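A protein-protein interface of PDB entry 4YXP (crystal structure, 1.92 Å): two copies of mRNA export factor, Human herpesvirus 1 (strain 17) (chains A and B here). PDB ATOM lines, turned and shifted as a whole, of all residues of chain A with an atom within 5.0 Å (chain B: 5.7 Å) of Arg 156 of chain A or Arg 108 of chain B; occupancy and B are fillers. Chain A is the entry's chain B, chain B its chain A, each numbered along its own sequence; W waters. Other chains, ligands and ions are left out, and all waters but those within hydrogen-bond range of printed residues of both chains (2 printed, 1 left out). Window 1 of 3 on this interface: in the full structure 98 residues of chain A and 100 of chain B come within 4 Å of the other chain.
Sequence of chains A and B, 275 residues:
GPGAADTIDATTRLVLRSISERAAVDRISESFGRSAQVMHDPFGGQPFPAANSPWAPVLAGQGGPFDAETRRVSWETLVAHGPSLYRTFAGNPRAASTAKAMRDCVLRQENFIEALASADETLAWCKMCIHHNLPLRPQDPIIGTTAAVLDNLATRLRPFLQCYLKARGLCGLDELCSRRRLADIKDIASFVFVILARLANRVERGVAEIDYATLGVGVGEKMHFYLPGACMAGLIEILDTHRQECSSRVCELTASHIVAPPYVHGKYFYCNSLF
Of the 13 printed residues of chain B, 6 touch a printed residue of chain A. Of the 13 printed residues of chain A, 5 touch a printed residue of chain B.
NH1 of Arg 108 of chain B lies within hydrogen-bond range of O of Thr 155 of chain A. OG1 of Thr 155 of chain A sits at hydrogen-bond distance from O of Asp 151 of chain B (3.5 Å). OD2 of Asp 151 of chain B lies within salt-bridge range of NE of Arg 158 of chain A (3.5 Å).
OD1 of Asn 152 of chain A lies within hydrogen-bond range of NE of Arg 156 of chain A. The backbone carbonyl oxygen (O) of Val 106 of chain B sits at hydrogen-bond distance from the side-chain amide nitrogen (NE2) of Gln 109 of chain B (3.0 Å). O of Glu 110 of chain B is in hydrogen-bond range of ND2 of Asn 152 of chain B (3.0 Å). The backbone carbonyl oxygen of Glu 110 of chain A is in hydrogen-bond range of the guanidinium group of Arg 156 of chain A, at 2.6 Å. ND2 of Asn 152 of chain B sits at hydrogen-bond distance from O of Leu 107 of chain B (2.9 Å). The guanidinium group (NH2) of Arg 156 of chain B lies within hydrogen-bond range of the backbone carbonyl oxygen (O) of Glu 110 of chain B (2.8 Å).
Gln 109 of chain A touches Arg 156 of chain B, and with the chains exchanged Arg 156 of chain A touches Gln 109 of chain B. Of the 9 pairs that touch across the chains among the printed residues, 2 have their exchanged pair printed and touching as well.
Water W1 lies within hydrogen-bond range of O of Gln 109 of chain B (2.7 Å) and NH2 of Arg 156 of chain A (3.0 Å). Water W2 lies within hydrogen-bond range of the guanidinium group (NH2) of Arg 156 of chain B and the backbone carbonyl oxygen (O) of Gln 109 of chain A.
Printed residues of chain B within 4 Å of Gln 109 of chain A: Arg 156 (3.1 Å). Of chain B, only Arg 108 (3.7 Å) and Gln 109 (3.3 Å) come within 4 Å of Arg 156 of chain A. Of the printed residues of chain B, Arg 158 of chain A touches Asp 151. Printed residues of chain A within 4 Å of Asp 104 of chain B: Pro 159. Of chain A, only Thr 155, Arg 156 and Pro 159 come within 4 Å of Arg 108 of chain B. Printed residues of chain A within 4 Å of Arg 156 of chain B: Gln 109. The nearest residue of chain B that does not touch Arg 156 of chain A is Arg 156 of chain B (4.4 Å). The nearest residue of chain A that does not touch Arg 108 of chain B is Arg 158 of chain A (4.2 Å). The nearest printed residue of chain A that does not touch Asp 151 of chain B is Ala 154 of chain A (5.4 Å).
Among the printed residues, merely in contact across the chains: Gln 109 of chain A with Arg 156 of chain B (3.1 Å), Pro 159 of chain A with Asp 104 of chain B (3.2 Å), Arg 156 of chain A with Gln 109 of chain B (3.3 Å), Pro 159 of chain A with Arg 108 of chain B (3.5 Å), Arg 156 of chain A with Arg 108 of chain B (3.7 Å) and Thr 155 of chain A with Asn 152 of chain B (3.9 Å).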
ATOM      1  N   GLN A 109      12.742  22.518  25.367  1.00  0.00           N
ATOM      2  CA  GLN A 109      12.330  21.606  24.295  1.00  0.00           C
ATOM      3  C   GLN A 109      10.810  21.542  24.093  1.00  0.00           C
ATOM      4  O   GLN A 109      10.325  20.731  23.305  1.00  0.00           O
ATOM      5  CB  GLN A 109      12.878  20.194  24.557  1.00  0.00           C
ATOM      6  CG  GLN A 109      12.386  19.522  25.835  1.00  0.00           C
ATOM      7  CD  GLN A 109      11.015  18.885  25.691  1.00  0.00           C
ATOM      8  OE1 GLN A 109      10.850  17.891  24.983  1.00  0.00           O
ATOM      9  NE2 GLN A 109      10.024  19.451  26.370  1.00  0.00           N
ATOM     10  N   GLU A 110      10.064  22.397  24.788  1.00  0.00           N
ATOM     11  CA  GLU A 110       8.603  22.422  24.650  1.00  0.00           C
ATOM     12  C   GLU A 110       8.156  22.946  23.287  1.00  0.00           C
ATOM     13  O   GLU A 110       8.858  23.749  22.670  1.00  0.00           O
ATOM     14  CB  GLU A 110       7.974  23.290  25.751  1.00  0.00           C
ATOM     15  CG  GLU A 110       7.868  22.605  27.090  1.00  0.00           C
ATOM     16  CD  GLU A 110       7.147  23.447  28.130  1.00  0.00           C
ATOM     17  OE1 GLU A 110       7.358  24.682  28.157  1.00  0.00           O
ATOM     18  OE2 GLU A 110       6.371  22.868  28.919  1.00  0.00           O
ATOM     19  N   ASN A 111       6.988  22.499  22.823  1.00  0.00           N
ATOM     20  CA  ASN A 111       6.431  23.009  21.567  1.00  0.00           C
ATOM     21  C   ASN A 111       5.799  24.376  21.828  1.00  0.00           C
ATOM     22  O   ASN A 111       5.778  24.841  22.967  1.00  0.00           O
ATOM     23  CB  ASN A 111       5.425  22.020  20.953  1.00  0.00           C
ATOM     24  CG  ASN A 111       4.142  21.867  21.765  1.00  0.00           C
ATOM     25  OD1 ASN A 111       3.726  22.761  22.495  1.00  0.00           O
ATOM     26  ND2 ASN A 111       3.498  20.715  21.616  1.00  0.00           N
ATOM     27  N   PHE A 112       5.299  25.031  20.782  1.00  0.00           N
ATOM     28  CA  PHE A 112       4.919  26.437  20.907  1.00  0.00           C
ATOM     29  C   PHE A 112       3.798  26.664  21.923  1.00  0.00           C
ATOM     30  O   PHE A 112       3.887  27.575  22.744  1.00  0.00           O
ATOM     31  CB  PHE A 112       4.503  27.009  19.551  1.00  0.00           C
ATOM     32  CG  PHE A 112       4.109  28.458  19.610  1.00  0.00           C
ATOM     33  CD1 PHE A 112       5.017  29.416  20.039  1.00  0.00           C
ATOM     34  CD2 PHE A 112       2.837  28.863  19.249  1.00  0.00           C
ATOM     35  CE1 PHE A 112       4.661  30.754  20.099  1.00  0.00           C
ATOM     36  CE2 PHE A 112       2.474  30.201  19.308  1.00  0.00           C
ATOM     37  CZ  PHE A 112       3.385  31.146  19.733  1.00  0.00           C
ATOM     38  N   ASN A 152      13.176  29.845  24.253  1.00  0.00           N
ATOM     39  CA  ASN A 152      12.337  29.005  23.411  1.00  0.00           C
ATOM     40  C   ASN A 152      11.363  29.840  22.573  1.00  0.00           C
ATOM     41  O   ASN A 152      11.260  29.650  21.358  1.00  0.00           O
ATOM     42  CB  ASN A 152      11.564  27.996  24.267  1.00  0.00           C
ATOM     43  CG  ASN A 152      11.085  26.799  23.463  1.00  0.00           C
ATOM     44  OD1 ASN A 152      11.571  26.539  22.360  1.00  0.00           O
ATOM     45  ND2 ASN A 152      10.138  26.059  24.014  1.00  0.00           N
ATOM     46  N   LEU A 153      10.652  30.763  23.214  1.00  0.00           N
ATOM     47  CA  LEU A 153       9.694  31.605  22.498  1.00  0.00           C
ATOM     48  C   LEU A 153      10.395  32.494  21.475  1.00  0.00           C
ATOM     49  O   LEU A 153       9.879  32.721  20.378  1.00  0.00           O
ATOM     50  CB  LEU A 153       8.888  32.473  23.471  1.00  0.00           C
ATOM     51  CG  LEU A 153       7.784  31.774  24.274  1.00  0.00           C
ATOM     52  CD1 LEU A 153       7.194  32.724  25.313  1.00  0.00           C
ATOM     53  CD2 LEU A 153       6.686  31.245  23.365  1.00  0.00           C
ATOM     54  N   ALA A 154      11.568  33.002  21.834  1.00  0.00           N
ATOM     55  CA  ALA A 154      12.333  33.848  20.927  1.00  0.00           C
ATOM     56  C   ALA A 154      12.770  33.068  19.685  1.00  0.00           C
ATOM     57  O   ALA A 154      12.708  33.578  18.567  1.00  0.00           O
ATOM     58  CB  ALA A 154      13.543  34.427  21.639  1.00  0.00           C
ATOM     59  N   THR A 155      13.217  31.833  19.888  1.00  0.00           N
ATOM     60  CA  THR A 155      13.651  30.989  18.780  1.00  0.00           C
ATOM     61  C   THR A 155      12.488  30.763  17.813  1.00  0.00           C
ATOM     62  O   THR A 155      12.654  30.826  16.598  1.00  0.00           O
ATOM     63  CB  THR A 155      14.198  29.630  19.291  1.00  0.00           C
ATOM     64  OG1 THR A 155      15.419  29.844  20.009  1.00  0.00           O
ATOM     65  CG2 THR A 155      14.464  28.660  18.135  1.00  0.00           C
ATOM     66  N   ARG A 156      11.303  30.523  18.356  1.00  0.00           N
ATOM     67  CA  ARG A 156      10.161  30.165  17.523  1.00  0.00           C
ATOM     68  C   ARG A 156       9.522  31.378  16.840  1.00  0.00           C
ATOM     69  O   ARG A 156       9.038  31.267  15.713  1.00  0.00           O
ATOM     70  CB  ARG A 156       9.132  29.406  18.370  1.00  0.00           C
ATOM     71  CG  ARG A 156       9.613  27.999  18.740  1.00  0.00           C
ATOM     72  CD  ARG A 156       8.835  27.355  19.891  1.00  0.00           C
ATOM     73  NE  ARG A 156       9.486  26.108  20.306  1.00  0.00           N
ATOM     74  CZ  ARG A 156       9.230  24.906  19.791  1.00  0.00           C
ATOM     75  NH1 ARG A 156       8.306  24.755  18.845  1.00  0.00           N
ATOM     76  NH2 ARG A 156       9.893  23.840  20.234  1.00  0.00           N
ATOM     77  N   LEU A 157       9.550  32.537  17.494  1.00  0.00           N
ATOM     78  CA  LEU A 157       8.822  33.706  16.991  1.00  0.00           C
ATOM     79  C   LEU A 157       9.681  34.759  16.281  1.00  0.00           C
ATOM     80  O   LEU A 157       9.142  35.719  15.734  1.00  0.00           O
ATOM     81  CB  LEU A 157       8.077  34.387  18.146  1.00  0.00           C
ATOM     82  CG  LEU A 157       6.897  33.629  18.759  1.00  0.00           C
ATOM     83  CD1 LEU A 157       6.395  34.357  19.996  1.00  0.00           C
ATOM     84  CD2 LEU A 157       5.767  33.447  17.757  1.00  0.00           C
ATOM     85  N   ARG A 158      11.001  34.589  16.271  1.00  0.00           N
ATOM     86  CA  ARG A 158      11.887  35.654  15.790  1.00  0.00           C
ATOM     87  C   ARG A 158      11.553  36.123  14.362  1.00  0.00           C
ATOM     88  O   ARG A 158      11.463  37.329  14.121  1.00  0.00           O
ATOM     89  CB  ARG A 158      13.355  35.211  15.872  1.00  0.00           C
ATOM     90  CG  ARG A 158      14.353  36.291  15.458  1.00  0.00           C
ATOM     91  CD  ARG A 158      15.794  35.830  15.636  1.00  0.00           C
ATOM     92  NE  ARG A 158      16.080  35.413  17.007  1.00  0.00           N
ATOM     93  CZ  ARG A 158      16.479  36.228  17.980  1.00  0.00           C
ATOM     94  NH1 ARG A 158      16.645  37.525  17.749  1.00  0.00           N
ATOM     95  NH2 ARG A 158      16.713  35.742  19.193  1.00  0.00           N
ATOM     96  N   PRO A 159      11.364  35.188  13.411  1.00  0.00           N
ATOM     97  CA  PRO A 159      11.059  35.654  12.048  1.00  0.00           C
ATOM     98  C   PRO A 159       9.713  36.368  11.931  1.00  0.00           C
ATOM     99  O   PRO A 159       9.590  37.324  11.165  1.00  0.00           O
ATOM    100  CB  PRO A 159      11.056  34.359  11.225  1.00  0.00           C
ATOM    101  CG  PRO A 159      11.869  33.403  12.026  1.00  0.00           C
ATOM    102  CD  PRO A 159      11.537  33.727  13.448  1.00  0.00           C
ATOM    103  N   ILE A 258       3.506  28.300  12.431  1.00  0.00           N
ATOM    104  CA  ILE A 258       3.728  28.346  13.873  1.00  0.00           C
ATOM    105  C   ILE A 258       2.460  27.878  14.586  1.00  0.00           C
ATOM    106  O   ILE A 258       2.519  27.085  15.527  1.00  0.00           O
ATOM    107  CB  ILE A 258       4.143  29.762  14.328  1.00  0.00           C
ATOM    108  CG1 ILE A 258       5.540  30.095  13.792  1.00  0.00           C
ATOM    109  CG2 ILE A 258       4.120  29.883  15.858  1.00  0.00           C
ATOM    110  CD1 ILE A 258       5.950  31.542  13.974  1.00  0.00           C
ATOM    111  N   ARG B 103      10.677  25.594   5.801  1.00  0.00           N
ATOM    112  CA  ARG B 103      11.830  24.942   6.416  1.00  0.00           C
ATOM    113  C   ARG B 103      12.286  25.696   7.662  1.00  0.00           C
ATOM    114  O   ARG B 103      12.682  25.087   8.662  1.00  0.00           O
ATOM    115  CB  ARG B 103      12.986  24.830   5.414  1.00  0.00           C
ATOM    116  CG  ARG B 103      14.273  24.275   6.021  1.00  0.00           C
ATOM    117  CD  ARG B 103      15.381  24.103   4.983  1.00  0.00           C
ATOM    118  NE  ARG B 103      16.645  23.738   5.627  1.00  0.00           N
ATOM    119  CZ  ARG B 103      17.084  22.494   5.803  1.00  0.00           C
ATOM    120  NH1 ARG B 103      16.378  21.456   5.373  1.00  0.00           N
ATOM    121  NH2 ARG B 103      18.239  22.285   6.416  1.00  0.00           N
ATOM    122  N   ASP B 104      12.227  27.022   7.600  1.00  0.00           N
ATOM    123  CA  ASP B 104      12.601  27.860   8.737  1.00  0.00           C
ATOM    124  C   ASP B 104      11.784  27.487   9.977  1.00  0.00           C
ATOM    125  O   ASP B 104      12.336  27.310  11.066  1.00  0.00           O
ATOM    126  CB  ASP B 104      12.408  29.339   8.385  1.00  0.00           C
ATOM    127  CG  ASP B 104      12.760  30.271   9.531  1.00  0.00           C
ATOM    128  OD1 ASP B 104      13.960  30.514   9.765  1.00  0.00           O
ATOM    129  OD2 ASP B 104      11.830  30.775  10.191  1.00  0.00           O
ATOM    130  N   CYS B 105      10.472  27.354   9.807  1.00  0.00           N
ATOM    131  CA  CYS B 105       9.594  26.972  10.914  1.00  0.00           C
ATOM    132  C   CYS B 105       9.893  25.557  11.407  1.00  0.00           C
ATOM    133  O   CYS B 105       9.921  25.314  12.613  1.00  0.00           O
ATOM    134  CB  CYS B 105       8.123  27.074  10.501  1.00  0.00           C
ATOM    135  SG  CYS B 105       7.526  28.764  10.259  1.00  0.00           S
ATOM    136  N   VAL B 106      10.111  24.625  10.483  1.00  0.00           N
ATOM    137  CA  VAL B 106      10.408  23.245  10.863  1.00  0.00           C
ATOM    138  C   VAL B 106      11.640  23.199  11.758  1.00  0.00           C
ATOM    139  O   VAL B 106      11.622  22.576  12.818  1.00  0.00           O
ATOM    140  CB  VAL B 106      10.608  22.343   9.629  1.00  0.00           C
ATOM    141  CG1 VAL B 106      11.057  20.938  10.047  1.00  0.00           C
ATOM    142  CG2 VAL B 106       9.327  22.261   8.815  1.00  0.00           C
ATOM    143  N   LEU B 107      12.712  23.853  11.330  1.00  0.00           N
ATOM    144  CA  LEU B 107      13.971  23.793  12.061  1.00  0.00           C
ATOM    145  C   LEU B 107      13.875  24.469  13.428  1.00  0.00           C
ATOM    146  O   LEU B 107      14.630  24.141  14.344  1.00  0.00           O
ATOM    147  CB  LEU B 107      15.091  24.429  11.243  1.00  0.00           C
ATOM    148  CG  LEU B 107      15.890  23.449  10.379  1.00  0.00           C
ATOM    149  CD1 LEU B 107      14.974  22.601   9.510  1.00  0.00           C
ATOM    150  CD2 LEU B 107      16.896  24.205   9.532  1.00  0.00           C
ATOM    151  N   ARG B 108      12.939  25.401  13.574  1.00  0.00           N
ATOM    152  CA  ARG B 108      12.805  26.125  14.836  1.00  0.00           C
ATOM    153  C   ARG B 108      11.980  25.344  15.863  1.00  0.00           C
ATOM    154  O   ARG B 108      11.946  25.719  17.035  1.00  0.00           O
ATOM    155  CB  ARG B 108      12.209  27.518  14.583  1.00  0.00           C
ATOM    156  CG  ARG B 108      13.238  28.471  13.954  1.00  0.00           C
ATOM    157  CD  ARG B 108      12.702  29.846  13.572  1.00  0.00           C
ATOM    158  NE  ARG B 108      13.745  30.615  12.889  1.00  0.00           N
ATOM    159  CZ  ARG B 108      14.699  31.312  13.502  1.00  0.00           C
ATOM    160  NH1 ARG B 108      14.746  31.377  14.829  1.00  0.00           N
ATOM    161  NH2 ARG B 108      15.610  31.956  12.785  1.00  0.00           N
ATOM    162  N   GLN B 109      11.356  24.242  15.444  1.00  0.00           N
ATOM    163  CA  GLN B 109      10.578  23.407  16.365  1.00  0.00           C
ATOM    164  C   GLN B 109      11.067  21.953  16.451  1.00  0.00           C
ATOM    165  O   GLN B 109      10.453  21.133  17.139  1.00  0.00           O
ATOM    166  CB  GLN B 109       9.090  23.426  15.972  1.00  0.00           C
ATOM    167  CG  GLN B 109       8.776  22.904  14.571  1.00  0.00           C
ATOM    168  CD  GLN B 109       8.599  21.396  14.524  1.00  0.00           C
ATOM    169  OE1 GLN B 109       7.675  20.848  15.129  1.00  0.00           O
ATOM    170  NE2 GLN B 109       9.482  20.719  13.802  1.00  0.00           N
ATOM    171  N   GLU B 110      12.171  21.637  15.775  1.00  0.00           N
ATOM    172  CA  GLU B 110      12.727  20.278  15.789  1.00  0.00           C
ATOM    173  C   GLU B 110      13.259  19.875  17.166  1.00  0.00           C
ATOM    174  O   GLU B 110      13.706  20.731  17.933  1.00  0.00           O
ATOM    175  CB  GLU B 110      13.853  20.157  14.755  1.00  0.00           C
ATOM    176  CG  GLU B 110      13.359  19.871  13.348  1.00  0.00           C
ATOM    177  CD  GLU B 110      14.484  19.688  12.345  1.00  0.00           C
ATOM    178  OE1 GLU B 110      15.561  20.305  12.519  1.00  0.00           O
ATOM    179  OE2 GLU B 110      14.278  18.922  11.380  1.00  0.00           O
ATOM    180  N   ALA B 147      20.269  30.078  10.252  1.00  0.00           N
ATOM    181  CA  ALA B 147      20.030  30.760  11.522  1.00  0.00           C
ATOM    182  C   ALA B 147      19.008  30.012  12.378  1.00  0.00           C
ATOM    183  O   ALA B 147      19.036  30.089  13.615  1.00  0.00           O
ATOM    184  CB  ALA B 147      19.566  32.191  11.270  1.00  0.00           C
ATOM    185  N   ALA B 148      18.107  29.288  11.723  1.00  0.00           N
ATOM    186  CA  ALA B 148      17.059  28.559  12.435  1.00  0.00           C
ATOM    187  C   ALA B 148      17.636  27.388  13.229  1.00  0.00           C
ATOM    188  O   ALA B 148      17.275  27.175  14.385  1.00  0.00           O
ATOM    189  CB  ALA B 148      16.008  28.066  11.462  1.00  0.00           C
ATOM    190  N   ASP B 151      19.777  28.785  16.101  1.00  0.00           N
ATOM    191  CA  ASP B 151      18.947  29.238  17.223  1.00  0.00           C
ATOM    192  C   ASP B 151      18.404  28.076  18.046  1.00  0.00           C
ATOM    193  O   ASP B 151      18.378  28.134  19.281  1.00  0.00           O
ATOM    194  CB  ASP B 151      17.778  30.087  16.711  1.00  0.00           C
ATOM    195  CG  ASP B 151      18.172  31.525  16.435  1.00  0.00           C
ATOM    196  OD1 ASP B 151      19.363  31.864  16.603  1.00  0.00           O
ATOM    197  OD2 ASP B 151      17.288  32.318  16.043  1.00  0.00           O
ATOM    198  N   ASN B 152      17.947  27.035  17.355  1.00  0.00           N
ATOM    199  CA  ASN B 152      17.431  25.838  18.007  1.00  0.00           C
ATOM    200  C   ASN B 152      18.511  25.203  18.878  1.00  0.00           C
ATOM    201  O   ASN B 152      18.288  24.934  20.060  1.00  0.00           O
ATOM    202  CB  ASN B 152      16.921  24.839  16.957  1.00  0.00           C
ATOM    203  CG  ASN B 152      16.338  23.573  17.572  1.00  0.00           C
ATOM    204  OD1 ASN B 152      16.885  23.017  18.523  1.00  0.00           O
ATOM    205  ND2 ASN B 152      15.227  23.115  17.027  1.00  0.00           N
ATOM    206  N   ARG B 156      18.829  24.939  23.196  1.00  0.00           N
ATOM    207  CA  ARG B 156      18.865  23.658  23.896  1.00  0.00           C
ATOM    208  C   ARG B 156      20.176  23.420  24.654  1.00  0.00           C
ATOM    209  O   ARG B 156      20.174  22.823  25.734  1.00  0.00           O
ATOM    210  CB  ARG B 156      18.610  22.525  22.895  1.00  0.00           C
ATOM    211  CG  ARG B 156      17.166  22.498  22.401  1.00  0.00           C
ATOM    212  CD  ARG B 156      16.954  21.598  21.195  1.00  0.00           C
ATOM    213  NE  ARG B 156      15.574  21.701  20.714  1.00  0.00           N
ATOM    214  CZ  ARG B 156      14.563  20.949  21.148  1.00  0.00           C
ATOM    215  NH1 ARG B 156      14.767  20.008  22.062  1.00  0.00           N
ATOM    216  NH2 ARG B 156      13.342  21.131  20.657  1.00  0.00           N
HETATM  217  O   HOH W   1       8.520  21.406  19.030  1.00  0.00           O
HETATM  218  O   HOH W   2      11.378  19.053  21.152  1.00  0.00           O
